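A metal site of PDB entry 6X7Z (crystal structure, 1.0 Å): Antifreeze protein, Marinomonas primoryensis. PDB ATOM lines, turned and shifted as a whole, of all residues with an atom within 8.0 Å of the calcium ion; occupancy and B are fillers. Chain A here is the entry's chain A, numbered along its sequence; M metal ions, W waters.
The backbone NH of Gly 55 is in hydrogen-bond range of the side-chain carboxylate of Asp 75. The side-chain carboxylate (OD1) of Asp 72 lies close to the side-chain amide nitrogen (NE2) of Gln 59 (3.0 Å).
Within 4 Å of the calcium ion: Gly 55, Asp 72 and Pro 73. The nearest printed residue that does not touch the calcium ion is Gln 59 (4.4 Å).
The calcium ion is bound by the backbone carbonyl oxygen (O) of Pro 73 (2.3 Å), water W3 (2.4 Å), water W2 (2.4 Å), the backbone carbonyl oxygen (O) of Gly 55 (2.4 Å), water W1 (2.4 Å), water W4 (2.4 Å) and the side-chain carboxylate (OD1) of Asp 72 (2.5 Å).
Water W4 bridges the backbone carbonyl oxygen of Gly 74 (2.8 Å) and the backbone carbonyl oxygen of Ala 53 (3.0 Å).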
ATOM      1  N   TYR A  12       4.501 -10.223  13.490  1.00  0.00           N
ATOM      2  CA  TYR A  12       3.502  -9.250  13.923  1.00  0.00           C
ATOM      3  C   TYR A  12       2.758  -9.801  15.142  1.00  0.00           C
ATOM      4  O   TYR A  12       2.363 -10.970  15.137  1.00  0.00           O
ATOM      5  CB  TYR A  12       2.510  -8.976  12.794  1.00  0.00           C
ATOM      6  CG  TYR A  12       1.318  -8.189  13.273  1.00  0.00           C
ATOM      7  CD1 TYR A  12       1.393  -6.809  13.492  1.00  0.00           C
ATOM      8  CD2 TYR A  12       0.128  -8.822  13.589  1.00  0.00           C
ATOM      9  CE1 TYR A  12       0.327  -6.108  14.005  1.00  0.00           C
ATOM     10  CE2 TYR A  12      -0.949  -8.124  14.100  1.00  0.00           C
ATOM     11  CZ  TYR A  12      -0.859  -6.760  14.326  1.00  0.00           C
ATOM     12  OH  TYR A  12      -1.882  -6.034  14.851  1.00  0.00           O
ATOM     13  N   VAL A  52      -3.062   0.412  13.366  1.00  0.00           N
ATOM     14  CA  VAL A  52      -2.397  -0.592  12.509  1.00  0.00           C
ATOM     15  C   VAL A  52      -3.052  -1.953  12.664  1.00  0.00           C
ATOM     16  O   VAL A  52      -3.007  -2.773  11.728  1.00  0.00           O
ATOM     17  CB  VAL A  52      -0.892  -0.685  12.760  1.00  0.00           C
ATOM     18  CG1 VAL A  52      -0.520  -1.560  13.944  1.00  0.00           C
ATOM     19  CG2 VAL A  52      -0.167  -1.174  11.498  1.00  0.00           C
ATOM     20  N   ALA A  53      -3.598  -2.229  13.849  1.00  0.00           N
ATOM     21  CA  ALA A  53      -4.041  -3.578  14.209  1.00  0.00           C
ATOM     22  C   ALA A  53      -5.471  -3.872  13.756  1.00  0.00           C
ATOM     23  O   ALA A  53      -5.950  -4.993  13.965  1.00  0.00           O
ATOM     24  CB  ALA A  53      -3.864  -3.777  15.706  1.00  0.00           C
ATOM     25  N   LYS A  54      -6.131  -2.900  13.120  1.00  0.00           N
ATOM     26  CA  LYS A  54      -7.532  -3.052  12.693  1.00  0.00           C
ATOM     27  C   LYS A  54      -7.614  -3.323  11.184  1.00  0.00           C
ATOM     28  O   LYS A  54      -6.773  -2.805  10.419  1.00  0.00           O
ATOM     29  CB  LYS A  54      -8.315  -1.816  13.142  1.00  0.00           C
ATOM     30  CG  LYS A  54      -8.970  -2.017  14.509  1.00  0.00           C
ATOM     31  CD  LYS A  54      -8.581  -1.145  15.705  1.00  0.00           C
ATOM     32  CE  LYS A  54      -9.347  -1.523  16.953  1.00  0.00           C
ATOM     33  NZ  LYS A  54     -10.826  -1.458  16.808  1.00  0.00           N
ATOM     34  N   GLY A  55      -8.568  -4.163  10.789  1.00  0.00           N
ATOM     35  CA  GLY A  55      -8.882  -4.368   9.387  1.00  0.00           C
ATOM     36  C   GLY A  55      -7.675  -4.770   8.585  1.00  0.00           C
ATOM     37  O   GLY A  55      -6.913  -5.656   8.972  1.00  0.00           O
ATOM     38  N   THR A  56      -7.505  -4.113   7.429  1.00  0.00           N
ATOM     39  CA  THR A  56      -6.394  -4.388   6.518  1.00  0.00           C
ATOM     40  C   THR A  56      -5.272  -3.361   6.654  1.00  0.00           C
ATOM     41  O   THR A  56      -4.433  -3.217   5.773  1.00  0.00           O
ATOM     42  CB  THR A  56      -6.888  -4.465   5.083  1.00  0.00           C
ATOM     43  OG1 THR A  56      -7.481  -3.218   4.691  1.00  0.00           O
ATOM     44  CG2 THR A  56      -7.919  -5.534   4.901  1.00  0.00           C
ATOM     45  N   HIS A  57      -5.237  -2.650   7.785  1.00  0.00           N
ATOM     46  CA  HIS A  57      -4.224  -1.615   7.939  1.00  0.00           C
ATOM     47  C   HIS A  57      -2.819  -2.181   7.995  1.00  0.00           C
ATOM     48  O   HIS A  57      -1.892  -1.536   7.500  1.00  0.00           O
ATOM     49  CB  HIS A  57      -4.534  -0.771   9.172  1.00  0.00           C
ATOM     50  CG  HIS A  57      -5.824  -0.052   9.022  1.00  0.00           C
ATOM     51  ND1 HIS A  57      -6.559   0.400  10.113  1.00  0.00           N
ATOM     52  CD2 HIS A  57      -6.549   0.291   7.939  1.00  0.00           C
ATOM     53  CE1 HIS A  57      -7.671   0.952   9.691  1.00  0.00           C
ATOM     54  NE2 HIS A  57      -7.683   0.933   8.379  1.00  0.00           N
ATOM     55  N   LEU A  58      -2.620  -3.375   8.559  1.00  0.00           N
ATOM     56  CA  LEU A  58      -1.280  -3.956   8.584  1.00  0.00           C
ATOM     57  C   LEU A  58      -0.784  -4.236   7.168  1.00  0.00           C
ATOM     58  O   LEU A  58       0.381  -3.984   6.849  1.00  0.00           O
ATOM     59  CB  LEU A  58      -1.273  -5.257   9.406  1.00  0.00           C
ATOM     60  CG  LEU A  58       0.055  -5.985   9.451  1.00  0.00           C
ATOM     61  CD1 LEU A  58       1.124  -5.185  10.180  1.00  0.00           C
ATOM     62  CD2 LEU A  58      -0.130  -7.374  10.089  1.00  0.00           C
ATOM     63  N   GLN A  59      -1.673  -4.782   6.345  1.00  0.00           N
ATOM     64  CA  GLN A  59      -1.352  -5.074   4.929  1.00  0.00           C
ATOM     65  C   GLN A  59      -0.915  -3.773   4.245  1.00  0.00           C
ATOM     66  O   GLN A  59       0.078  -3.781   3.481  1.00  0.00           O
ATOM     67  CB  GLN A  59      -2.573  -5.643   4.214  1.00  0.00           C
ATOM     68  CG  GLN A  59      -2.854  -7.100   4.535  1.00  0.00           C
ATOM     69  CD  GLN A  59      -3.598  -7.362   5.835  1.00  0.00           C
ATOM     70  OE1 GLN A  59      -3.858  -6.463   6.638  1.00  0.00           O
ATOM     71  NE2 GLN A  59      -3.932  -8.626   6.051  1.00  0.00           N
ATOM     72  N   LEU A  69       2.780 -12.306   4.098  1.00  0.00           N
ATOM     73  CA  LEU A  69       2.098 -12.584   5.362  1.00  0.00           C
ATOM     74  C   LEU A  69       1.643 -14.042   5.410  1.00  0.00           C
ATOM     75  O   LEU A  69       1.013 -14.555   4.463  1.00  0.00           O
ATOM     76  CB  LEU A  69       0.880 -11.675   5.527  1.00  0.00           C
ATOM     77  CG  LEU A  69       1.195 -10.279   6.050  1.00  0.00           C
ATOM     78  CD1 LEU A  69       0.039  -9.328   5.801  1.00  0.00           C
ATOM     79  CD2 LEU A  69       1.536 -10.305   7.519  1.00  0.00           C
ATOM     80  N   THR A  71      -0.735 -15.109   7.437  1.00  0.00           N
ATOM     81  CA  THR A  71      -2.164 -15.079   7.705  1.00  0.00           C
ATOM     82  C   THR A  71      -2.564 -13.603   7.737  1.00  0.00           C
ATOM     83  O   THR A  71      -1.707 -12.722   7.822  1.00  0.00           O
ATOM     84  CB  THR A  71      -2.469 -15.838   9.003  1.00  0.00           C
ATOM     85  OG1 THR A  71      -3.862 -16.078   9.109  1.00  0.00           O
ATOM     86  CG2 THR A  71      -1.915 -15.098  10.187  1.00  0.00           C
ATOM     87  N   ASP A  72      -3.879 -13.358   7.708  1.00  0.00           N
ATOM     88  CA  ASP A  72      -4.448 -12.035   7.929  1.00  0.00           C
ATOM     89  C   ASP A  72      -4.907 -11.971   9.379  1.00  0.00           C
ATOM     90  O   ASP A  72      -5.914 -12.601   9.730  1.00  0.00           O
ATOM     91  CB  ASP A  72      -5.638 -11.820   7.003  1.00  0.00           C
ATOM     92  CG  ASP A  72      -6.353 -10.488   7.194  1.00  0.00           C
ATOM     93  OD1 ASP A  72      -5.867  -9.680   8.026  1.00  0.00           O
ATOM     94  OD2 ASP A  72      -7.390 -10.297   6.512  1.00  0.00           O
ATOM     95  N   PRO A  73      -4.174 -11.284  10.276  1.00  0.00           N
ATOM     96  CA  PRO A  73      -4.607 -11.209  11.666  1.00  0.00           C
ATOM     97  C   PRO A  73      -6.001 -10.661  11.805  1.00  0.00           C
ATOM     98  O   PRO A  73      -6.440  -9.809  11.030  1.00  0.00           O
ATOM     99  CB  PRO A  73      -3.576 -10.279  12.317  1.00  0.00           C
ATOM    100  CG  PRO A  73      -2.415 -10.214  11.392  1.00  0.00           C
ATOM    101  CD  PRO A  73      -2.986 -10.447  10.008  1.00  0.00           C
ATOM    102  N   GLY A  74      -6.697 -11.085  12.859  1.00  0.00           N
ATOM    103  CA  GLY A  74      -7.920 -10.439  13.239  1.00  0.00           C
ATOM    104  C   GLY A  74      -7.676  -9.057  13.855  1.00  0.00           C
ATOM    105  O   GLY A  74      -6.544  -8.606  13.985  1.00  0.00           O
ATOM    106  N   ASP A  75      -8.767  -8.384  14.212  1.00  0.00           N
ATOM    107  CA  ASP A  75      -8.639  -7.054  14.786  1.00  0.00           C
ATOM    108  C   ASP A  75      -8.038  -7.117  16.189  1.00  0.00           C
ATOM    109  O   ASP A  75      -8.373  -7.994  17.007  1.00  0.00           O
ATOM    110  CB  ASP A  75     -10.004  -6.377  14.902  1.00  0.00           C
ATOM    111  CG  ASP A  75     -10.577  -5.849  13.610  1.00  0.00           C
ATOM    112  OD1 ASP A  75      -9.914  -5.924  12.556  1.00  0.00           O
ATOM    113  OD2 ASP A  75     -11.733  -5.365  13.684  1.00  0.00           O
ATOM    114  N   ASN A  76      -7.238  -6.098  16.483  1.00  0.00           N
ATOM    115  CA  ASN A  76      -6.795  -5.768  17.831  1.00  0.00           C
ATOM    116  C   ASN A  76      -6.769  -4.240  17.934  1.00  0.00           C
ATOM    117  O   ASN A  76      -6.804  -3.553  16.919  1.00  0.00           O
ATOM    118  CB  ASN A  76      -5.368  -6.372  18.044  1.00  0.00           C
ATOM    119  CG  ASN A  76      -5.401  -7.811  18.514  1.00  0.00           C
ATOM    120  OD1 ASN A  76      -5.965  -8.168  19.610  1.00  0.00           O
ATOM    121  ND2 ASN A  76      -4.822  -8.644  17.769  1.00  0.00           N
HETATM  122 CA    CA M   1      -6.731  -7.979   9.597  1.00  0.00          CA
HETATM  123  O   HOH W   1      -4.449  -7.260   9.245  1.00  0.00           O
HETATM  124  O   HOH W   2      -8.843  -7.744  10.708  1.00  0.00           O
HETATM  125  O   HOH W   3      -8.246  -8.056   7.786  1.00  0.00           O
HETATM  126  O   HOH W   4      -6.034  -7.025  11.710  1.00  0.00           O
